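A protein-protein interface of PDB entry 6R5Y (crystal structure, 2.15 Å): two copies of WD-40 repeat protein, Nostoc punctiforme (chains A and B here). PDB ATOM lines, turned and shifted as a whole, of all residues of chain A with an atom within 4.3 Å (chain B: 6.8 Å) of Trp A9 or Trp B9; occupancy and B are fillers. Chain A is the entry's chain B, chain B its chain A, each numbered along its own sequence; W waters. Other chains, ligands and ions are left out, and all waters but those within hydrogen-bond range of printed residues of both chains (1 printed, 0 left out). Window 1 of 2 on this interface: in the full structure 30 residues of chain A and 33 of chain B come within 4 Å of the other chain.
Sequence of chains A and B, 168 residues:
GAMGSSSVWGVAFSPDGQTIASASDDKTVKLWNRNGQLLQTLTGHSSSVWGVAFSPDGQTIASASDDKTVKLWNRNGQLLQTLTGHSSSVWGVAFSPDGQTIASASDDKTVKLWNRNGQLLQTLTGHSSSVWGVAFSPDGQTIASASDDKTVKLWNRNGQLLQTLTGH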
ATOM      1  N   VAL A   8     -22.381   9.339  -0.077  1.00  0.00           N
ATOM      2  CA  VAL A   8     -22.735   7.972  -0.370  1.00  0.00           C
ATOM      3  C   VAL A   8     -23.861   7.471   0.527  1.00  0.00           C
ATOM      4  O   VAL A   8     -24.161   8.032   1.570  1.00  0.00           O
ATOM      5  CB  VAL A   8     -21.539   7.016  -0.177  1.00  0.00           C
ATOM      6  CG1 VAL A   8     -20.369   7.518  -0.992  1.00  0.00           C
ATOM      7  CG2 VAL A   8     -21.164   6.860   1.291  1.00  0.00           C
ATOM      8  N   TRP A   9     -24.475   6.388   0.111  1.00  0.00           N
ATOM      9  CA  TRP A   9     -25.684   5.953   0.771  1.00  0.00           C
ATOM     10  C   TRP A   9     -25.360   5.317   2.106  1.00  0.00           C
ATOM     11  O   TRP A   9     -24.512   4.432   2.180  1.00  0.00           O
ATOM     12  CB  TRP A   9     -26.386   4.985  -0.132  1.00  0.00           C
ATOM     13  CG  TRP A   9     -27.661   4.503   0.348  1.00  0.00           C
ATOM     14  CD1 TRP A   9     -27.985   3.238   0.778  1.00  0.00           C
ATOM     15  CD2 TRP A   9     -28.851   5.263   0.403  1.00  0.00           C
ATOM     16  NE1 TRP A   9     -29.314   3.176   1.081  1.00  0.00           N
ATOM     17  CE2 TRP A   9     -29.874   4.411   0.862  1.00  0.00           C
ATOM     18  CE3 TRP A   9     -29.165   6.590   0.071  1.00  0.00           C
ATOM     19  CZ2 TRP A   9     -31.186   4.858   1.048  1.00  0.00           C
ATOM     20  CZ3 TRP A   9     -30.479   7.030   0.249  1.00  0.00           C
ATOM     21  CH2 TRP A   9     -31.468   6.163   0.728  1.00  0.00           C
ATOM     22  N   GLY A  10     -26.061   5.758   3.149  1.00  0.00           N
ATOM     23  CA  GLY A  10     -25.705   5.423   4.528  1.00  0.00           C
ATOM     24  C   GLY A  10     -26.779   4.698   5.313  1.00  0.00           C
ATOM     25  O   GLY A  10     -26.839   4.828   6.520  1.00  0.00           O
ATOM     26  N   VAL A  11     -27.615   3.932   4.639  1.00  0.00           N
ATOM     27  CA  VAL A  11     -28.767   3.299   5.270  1.00  0.00           C
ATOM     28  C   VAL A  11     -28.862   1.886   4.732  1.00  0.00           C
ATOM     29  O   VAL A  11     -28.702   1.703   3.551  1.00  0.00           O
ATOM     30  CB  VAL A  11     -30.084   4.095   4.972  1.00  0.00           C
ATOM     31  CG1 VAL A  11     -31.312   3.288   5.290  1.00  0.00           C
ATOM     32  CG2 VAL A  11     -30.104   5.387   5.772  1.00  0.00           C
ATOM     33  N   TRP A  50     -19.528   5.824   6.906  1.00  0.00           N
ATOM     34  CA  TRP A  50     -20.162   6.169   5.639  1.00  0.00           C
ATOM     35  C   TRP A  50     -21.182   5.140   5.121  1.00  0.00           C
ATOM     36  O   TRP A  50     -22.176   5.507   4.540  1.00  0.00           O
ATOM     37  CB  TRP A  50     -19.086   6.375   4.596  1.00  0.00           C
ATOM     38  CG  TRP A  50     -18.118   7.496   4.928  1.00  0.00           C
ATOM     39  CD1 TRP A  50     -16.787   7.390   5.054  1.00  0.00           C
ATOM     40  CD2 TRP A  50     -18.440   8.867   5.193  1.00  0.00           C
ATOM     41  NE1 TRP A  50     -16.232   8.612   5.362  1.00  0.00           N
ATOM     42  CE2 TRP A  50     -17.230   9.537   5.468  1.00  0.00           C
ATOM     43  CE3 TRP A  50     -19.625   9.591   5.226  1.00  0.00           C
ATOM     44  CZ2 TRP A  50     -17.169  10.910   5.769  1.00  0.00           C
ATOM     45  CZ3 TRP A  50     -19.563  10.969   5.512  1.00  0.00           C
ATOM     46  CH2 TRP A  50     -18.345  11.602   5.786  1.00  0.00           C
ATOM     47  N   GLY A  51     -20.909   3.861   5.280  1.00  0.00           N
ATOM     48  CA  GLY A  51     -21.731   2.848   4.673  1.00  0.00           C
ATOM     49  C   GLY A  51     -22.068   1.758   5.666  1.00  0.00           C
ATOM     50  O   GLY A  51     -21.290   1.475   6.571  1.00  0.00           O
ATOM     51  N   TRP A 132     -16.809   4.021  -4.655  1.00  0.00           N
ATOM     52  CA  TRP A 132     -17.808   4.415  -3.672  1.00  0.00           C
ATOM     53  C   TRP A 132     -18.934   3.381  -3.464  1.00  0.00           C
ATOM     54  O   TRP A 132     -19.530   3.348  -2.389  1.00  0.00           O
ATOM     55  CB  TRP A 132     -18.418   5.776  -4.008  1.00  0.00           C
ATOM     56  CG  TRP A 132     -19.004   5.904  -5.370  1.00  0.00           C
ATOM     57  CD1 TRP A 132     -18.424   6.481  -6.484  1.00  0.00           C
ATOM     58  CD2 TRP A 132     -20.334   5.548  -5.768  1.00  0.00           C
ATOM     59  NE1 TRP A 132     -19.291   6.449  -7.546  1.00  0.00           N
ATOM     60  CE2 TRP A 132     -20.478   5.902  -7.136  1.00  0.00           C
ATOM     61  CE3 TRP A 132     -21.415   4.976  -5.109  1.00  0.00           C
ATOM     62  CZ2 TRP A 132     -21.660   5.677  -7.850  1.00  0.00           C
ATOM     63  CZ3 TRP A 132     -22.576   4.760  -5.820  1.00  0.00           C
ATOM     64  CH2 TRP A 132     -22.694   5.122  -7.170  1.00  0.00           C
ATOM     65  N   GLY A 133     -19.163   2.519  -4.458  1.00  0.00           N
ATOM     66  CA  GLY A 133     -20.229   1.533  -4.391  1.00  0.00           C
ATOM     67  C   GLY A 133     -19.813   0.139  -4.808  1.00  0.00           C
ATOM     68  O   GLY A 133     -18.914  -0.042  -5.642  1.00  0.00           O
ATOM     69  N   ALA A 146     -18.693   0.601  -8.459  1.00  0.00           N
ATOM     70  CA  ALA A 146     -18.910   1.906  -9.082  1.00  0.00           C
ATOM     71  C   ALA A 146     -17.934   2.922  -8.495  1.00  0.00           C
ATOM     72  O   ALA A 146     -17.704   2.946  -7.295  1.00  0.00           O
ATOM     73  CB  ALA A 146     -20.316   2.376  -8.834  1.00  0.00           C
ATOM     74  N   GLY B   4     -35.866  -4.129  -2.203  1.00  0.00           N
ATOM     75  CA  GLY B   4     -36.140  -3.179  -3.294  1.00  0.00           C
ATOM     76  C   GLY B   4     -35.047  -3.225  -4.385  1.00  0.00           C
ATOM     77  O   GLY B   4     -34.237  -4.147  -4.446  1.00  0.00           O
ATOM     78  N   SER B   5     -35.063  -2.259  -5.288  1.00  0.00           N
ATOM     79  CA  SER B   5     -33.903  -2.009  -6.151  1.00  0.00           C
ATOM     80  C   SER B   5     -33.744  -0.493  -6.264  1.00  0.00           C
ATOM     81  O   SER B   5     -34.730   0.235  -6.313  1.00  0.00           O
ATOM     82  CB  SER B   5     -34.097  -2.672  -7.501  1.00  0.00           C
ATOM     83  OG  SER B   5     -35.201  -2.056  -8.155  1.00  0.00           O
ATOM     84  N   SER B   6     -32.509  -0.015  -6.223  1.00  0.00           N
ATOM     85  CA  SER B   6     -32.262   1.410  -6.194  1.00  0.00           C
ATOM     86  C   SER B   6     -31.000   1.789  -6.940  1.00  0.00           C
ATOM     87  O   SER B   6     -30.059   0.990  -7.010  1.00  0.00           O
ATOM     88  CB  SER B   6     -32.193   1.920  -4.744  1.00  0.00           C
ATOM     89  OG  SER B   6     -31.892   3.303  -4.682  1.00  0.00           O
ATOM     90  N   SER B   7     -30.973   3.039  -7.425  1.00  0.00           N
ATOM     91  CA  SER B   7     -29.811   3.634  -8.056  1.00  0.00           C
ATOM     92  C   SER B   7     -28.717   4.049  -7.044  1.00  0.00           C
ATOM     93  O   SER B   7     -27.665   4.507  -7.437  1.00  0.00           O
ATOM     94  CB  SER B   7     -30.221   4.828  -8.930  1.00  0.00           C
ATOM     95  OG  SER B   7     -30.703   5.871  -8.127  1.00  0.00           O
ATOM     96  N   VAL B   8     -28.939   3.881  -5.741  1.00  0.00           N
ATOM     97  CA  VAL B   8     -28.034   4.537  -4.786  1.00  0.00           C
ATOM     98  C   VAL B   8     -26.646   3.902  -4.634  1.00  0.00           C
ATOM     99  O   VAL B   8     -25.750   4.589  -4.172  1.00  0.00           O
ATOM    100  CB  VAL B   8     -28.644   4.789  -3.366  1.00  0.00           C
ATOM    101  CG1 VAL B   8     -29.813   5.757  -3.405  1.00  0.00           C
ATOM    102  CG2 VAL B   8     -29.028   3.495  -2.660  1.00  0.00           C
ATOM    103  N   TRP B   9     -26.468   2.652  -5.066  1.00  0.00           N
ATOM    104  CA  TRP B   9     -25.196   1.920  -4.992  1.00  0.00           C
ATOM    105  C   TRP B   9     -24.443   1.974  -6.309  1.00  0.00           C
ATOM    106  O   TRP B   9     -23.339   1.448  -6.395  1.00  0.00           O
ATOM    107  CB  TRP B   9     -25.432   0.450  -4.583  1.00  0.00           C
ATOM    108  CG  TRP B   9     -26.090   0.365  -3.269  1.00  0.00           C
ATOM    109  CD1 TRP B   9     -25.499   0.604  -2.066  1.00  0.00           C
ATOM    110  CD2 TRP B   9     -27.459   0.080  -3.002  1.00  0.00           C
ATOM    111  NE1 TRP B   9     -26.406   0.482  -1.064  1.00  0.00           N
ATOM    112  CE2 TRP B   9     -27.625   0.158  -1.602  1.00  0.00           C
ATOM    113  CE3 TRP B   9     -28.568  -0.237  -3.800  1.00  0.00           C
ATOM    114  CZ2 TRP B   9     -28.864  -0.083  -0.965  1.00  0.00           C
ATOM    115  CZ3 TRP B   9     -29.815  -0.462  -3.161  1.00  0.00           C
ATOM    116  CH2 TRP B   9     -29.939  -0.390  -1.763  1.00  0.00           C
ATOM    117  N   GLY B  10     -25.040   2.583  -7.334  1.00  0.00           N
ATOM    118  CA  GLY B  10     -24.412   2.759  -8.636  1.00  0.00           C
ATOM    119  C   GLY B  10     -24.381   1.563  -9.559  1.00  0.00           C
ATOM    120  O   GLY B  10     -23.692   1.584 -10.559  1.00  0.00           O
ATOM    121  N   VAL B  11     -25.136   0.530  -9.235  1.00  0.00           N
ATOM    122  CA  VAL B  11     -25.124  -0.680 -10.010  1.00  0.00           C
ATOM    123  C   VAL B  11     -26.542  -1.151 -10.146  1.00  0.00           C
ATOM    124  O   VAL B  11     -27.315  -1.043  -9.200  1.00  0.00           O
ATOM    125  CB  VAL B  11     -24.297  -1.777  -9.320  1.00  0.00           C
ATOM    126  CG1 VAL B  11     -24.604  -3.151  -9.932  1.00  0.00           C
ATOM    127  CG2 VAL B  11     -22.841  -1.474  -9.453  1.00  0.00           C
ATOM    128  N   ALA B  12     -26.918  -1.609 -11.334  1.00  0.00           N
ATOM    129  CA  ALA B  12     -28.278  -2.093 -11.550  1.00  0.00           C
ATOM    130  C   ALA B  12     -28.130  -3.386 -12.346  1.00  0.00           C
ATOM    131  O   ALA B  12     -27.940  -3.391 -13.572  1.00  0.00           O
ATOM    132  CB  ALA B  12     -29.184  -1.051 -12.203  1.00  0.00           C
ATOM    133  N   TRP B 132     -30.871  13.275  -3.333  1.00  0.00           N
ATOM    134  CA  TRP B 132     -30.106  12.549  -4.342  1.00  0.00           C
ATOM    135  C   TRP B 132     -30.350  11.049  -4.337  1.00  0.00           C
ATOM    136  O   TRP B 132     -30.077  10.375  -5.324  1.00  0.00           O
ATOM    137  CB  TRP B 132     -28.604  12.853  -4.208  1.00  0.00           C
ATOM    138  CG  TRP B 132     -28.030  12.661  -2.870  1.00  0.00           C
ATOM    139  CD1 TRP B 132     -27.813  13.637  -1.914  1.00  0.00           C
ATOM    140  CD2 TRP B 132     -27.536  11.447  -2.328  1.00  0.00           C
ATOM    141  NE1 TRP B 132     -27.232  13.087  -0.816  1.00  0.00           N
ATOM    142  CE2 TRP B 132     -27.058  11.740  -1.040  1.00  0.00           C
ATOM    143  CE3 TRP B 132     -27.455  10.129  -2.801  1.00  0.00           C
ATOM    144  CZ2 TRP B 132     -26.496  10.764  -0.217  1.00  0.00           C
ATOM    145  CZ3 TRP B 132     -26.886   9.151  -1.979  1.00  0.00           C
ATOM    146  CH2 TRP B 132     -26.411   9.480  -0.711  1.00  0.00           C
ATOM    147  N   GLY B 133     -30.799  10.521  -3.209  1.00  0.00           N
ATOM    148  CA  GLY B 133     -30.930   9.084  -3.035  1.00  0.00           C
ATOM    149  C   GLY B 133     -32.246   8.698  -2.419  1.00  0.00           C
ATOM    150  O   GLY B 133     -32.769   9.413  -1.560  1.00  0.00           O
ATOM    151  N   VAL B 134     -32.784   7.572  -2.870  1.00  0.00           N
ATOM    152  CA  VAL B 134     -34.003   7.021  -2.295  1.00  0.00           C
ATOM    153  C   VAL B 134     -33.996   5.495  -2.395  1.00  0.00           C
ATOM    154  O   VAL B 134     -33.430   4.940  -3.328  1.00  0.00           O
ATOM    155  CB  VAL B 134     -35.235   7.596  -3.005  1.00  0.00           C
ATOM    156  CG1 VAL B 134     -35.296   7.152  -4.468  1.00  0.00           C
ATOM    157  CG2 VAL B 134     -36.494   7.211  -2.259  1.00  0.00           C
ATOM    158  N   ALA B 135     -34.544   4.820  -1.375  1.00  0.00           N
ATOM    159  CA  ALA B 135     -34.637   3.393  -1.362  1.00  0.00           C
ATOM    160  C   ALA B 135     -35.844   2.920  -0.533  1.00  0.00           C
ATOM    161  O   ALA B 135     -36.179   3.541   0.491  1.00  0.00           O
ATOM    162  CB  ALA B 135     -33.346   2.786  -0.814  1.00  0.00           C
ATOM    163  N   PHE B 136     -36.425   1.798  -0.941  1.00  0.00           N
ATOM    164  CA  PHE B 136     -37.464   1.116  -0.165  1.00  0.00           C
ATOM    165  C   PHE B 136     -36.929   0.081   0.794  1.00  0.00           C
ATOM    166  O   PHE B 136     -35.856  -0.476   0.571  1.00  0.00           O
ATOM    167  CB  PHE B 136     -38.387   0.324  -1.057  1.00  0.00           C
ATOM    168  CG  PHE B 136     -39.278   1.158  -1.865  1.00  0.00           C
ATOM    169  CD1 PHE B 136     -38.841   1.673  -3.067  1.00  0.00           C
ATOM    170  CD2 PHE B 136     -40.547   1.454  -1.410  1.00  0.00           C
ATOM    171  CE1 PHE B 136     -39.665   2.474  -3.810  1.00  0.00           C
ATOM    172  CE2 PHE B 136     -41.376   2.225  -2.153  1.00  0.00           C
ATOM    173  CZ  PHE B 136     -40.933   2.747  -3.354  1.00  0.00           C
ATOM    174  N   ALA B 144     -36.600   5.318   2.631  1.00  0.00           N
ATOM    175  CA  ALA B 144     -35.509   6.168   3.095  1.00  0.00           C
ATOM    176  C   ALA B 144     -35.033   7.094   1.965  1.00  0.00           C
ATOM    177  O   ALA B 144     -34.918   6.660   0.819  1.00  0.00           O
ATOM    178  CB  ALA B 144     -34.349   5.332   3.572  1.00  0.00           C
ATOM    179  N   SER B 145     -34.752   8.358   2.306  1.00  0.00           N
ATOM    180  CA  SER B 145     -34.231   9.355   1.347  1.00  0.00           C
ATOM    181  C   SER B 145     -33.034  10.079   1.953  1.00  0.00           C
ATOM    182  O   SER B 145     -33.000  10.340   3.141  1.00  0.00           O
ATOM    183  CB  SER B 145     -35.306  10.393   0.984  1.00  0.00           C
ATOM    184  OG  SER B 145     -35.793  11.044   2.144  1.00  0.00           O
ATOM    185  N   ALA B 146     -32.096  10.462   1.099  1.00  0.00           N
ATOM    186  CA  ALA B 146     -30.902  11.162   1.507  1.00  0.00           C
ATOM    187  C   ALA B 146     -30.782  12.443   0.691  1.00  0.00           C
ATOM    188  O   ALA B 146     -30.944  12.410  -0.520  1.00  0.00           O
ATOM    189  CB  ALA B 146     -29.681  10.281   1.267  1.00  0.00           C
ATOM    190  N   SER B 147     -30.419  13.518   1.369  1.00  0.00           N
ATOM    191  CA  SER B 147     -30.385  14.848   0.816  1.00  0.00           C
ATOM    192  C   SER B 147     -29.053  15.592   1.052  1.00  0.00           C
ATOM    193  O   SER B 147     -28.273  15.236   1.921  1.00  0.00           O
ATOM    194  CB  SER B 147     -31.474  15.623   1.495  1.00  0.00           C
ATOM    195  OG  SER B 147     -31.458  16.975   1.121  1.00  0.00           O
ATOM    196  N   VAL B 152     -30.942  12.197   6.496  1.00  0.00           N
ATOM    197  CA  VAL B 152     -31.617  11.046   5.961  1.00  0.00           C
ATOM    198  C   VAL B 152     -32.943  11.034   6.653  1.00  0.00           C
ATOM    199  O   VAL B 152     -33.017  11.160   7.866  1.00  0.00           O
ATOM    200  CB  VAL B 152     -30.881   9.716   6.242  1.00  0.00           C
ATOM    201  CG1 VAL B 152     -31.664   8.530   5.678  1.00  0.00           C
ATOM    202  CG2 VAL B 152     -29.481   9.755   5.631  1.00  0.00           C
ATOM    203  N   LYS B 153     -33.988  10.843   5.875  1.00  0.00           N
ATOM    204  CA  LYS B 153     -35.339  10.811   6.407  1.00  0.00           C
ATOM    205  C   LYS B 153     -35.970   9.470   6.096  1.00  0.00           C
ATOM    206  O   LYS B 153     -35.797   8.904   5.013  1.00  0.00           O
ATOM    207  CB  LYS B 153     -36.167  11.967   5.829  1.00  0.00           C
ATOM    208  CG  LYS B 153     -35.768  13.308   6.420  1.00  0.00           C
ATOM    209  CD  LYS B 153     -36.528  14.472   5.805  1.00  0.00           C
ATOM    210  CE  LYS B 153     -36.040  15.799   6.356  1.00  0.00           C
ATOM    211  NZ  LYS B 153     -36.503  16.015   7.744  1.00  0.00           N
HETATM  212  O   HOH W   1     -23.767   5.073  -2.384  1.00  0.00           O
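The backbone carbonyl oxygen of Gly A133 is in hydrogen-bond range of the backbone NH of Ala A146, at 2.9 Å.
The backbone carbonyl oxygen of Ala A146 lies within hydrogen-bond range of the backbone NH of Trp A132.
The backbone carbonyl oxygen of Val A11 is in hydrogen-bond range of the indole nitrogen of Trp A9 (2.9 Å).
The backbone NH (N) of Trp B132 sits at hydrogen-bond distance from the backbone carbonyl oxygen (O) of Ala B146, 2.9 Å away.
N of Ala B144 is in hydrogen-bond range of O of Ala B135 (2.8 Å).
OG of Ser B6 sits at hydrogen-bond distance from O of Val B134, at 2.6 Å.
Trp A9 touches Val B8 (CG to CG2, 3.5 Å).
Trp A9 touches Trp B9 (CD1 to NE1, 3.7 Å).
Trp B132 touches Trp A9.
Gly B133 touches Trp A9 (C to CZ3, 3.6 Å).
Trp A9 touches Val B134 (CZ3 to N, 3.9 Å).
CZ2 of Trp A9 touches CB of Ala B135 (3.5 Å).
CB of Ala B146 touches CZ3 of Trp A9, at 3.5 Å.
Val B152 touches Val A11 (CG1 to CG2, 3.5 Å).
Gly A133 touches Trp B9 (CA to O, 3.7 Å).
Ala A146 touches Gly B10.
Of the printed residues of chain B, Val A8 touches Trp B132.
Trp A9 touches eight residues of chain B.
Gly A51 touches none of the printed residues of chain B.
Of the printed residues of chain B, Gly A133 touches Trp B9.
Of the printed residues of chain A, Trp B9 touches Trp A9 (3.7 Å), Trp A132 (3.4 Å), Gly A133 (3.7 Å) and Ala A146 (3.99 Å).
Of the printed residues of chain A, Ala B135 touches Trp A9 (3.5 Å).
Of the printed residues of chain A, Ala B146 touches Trp A9.
The nearest residue of chain B that does not touch Trp A9 is Ser B145 (4.3 Å).
The nearest printed residue of chain A that does not touch Trp B9 is Val A11 (4.9 Å).
The nearest printed residue of chain A that does not touch Gly B133 is Val A8 (8.1 Å).
Of the 9 printed residues of chain A, 6 touch a printed residue of chain B.
Printed residues of chain A that touch a printed residue of chain B: Val A8, Trp A9, Val A11, Trp A132, Gly A133 and Ala A146.
Hydrophobic or aromatic side chains of chain A within 4 Å of the printed part of chain B: Trp A9, Val A11, Trp A132 and Ala A146.
Printed residues of chain B that touch a printed residue of chain A: Val B8, Trp B9, Gly B10, Trp B132, Gly B133, Val B134, Ala B135, Ala B144, Ala B146 and Val B152.
Hydrophobic or aromatic side chains of chain B that line the printed part of chain A: Val B8, Trp B9, Trp B132, Ala B135, Ala B146 and Val B152.
Val A8 touches Trp B132, and with the chains exchanged Trp A132 touches Val B8.
Trp A9 touches Val B8, but with the chains exchanged Val A8 does not touch Trp B9 (7.5 Å).
Trp A132 touches Gly B10, but with the chains exchanged Gly A10 does not touch Trp B132 (5.4 Å).
Ala A146 touches Gly B10, but with the chains exchanged Gly A10 does not touch Ala B146 (6.1 Å).
Water W1 bridges O of Val B8 (2.7 Å) and N of Trp A9 (2.9 Å).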
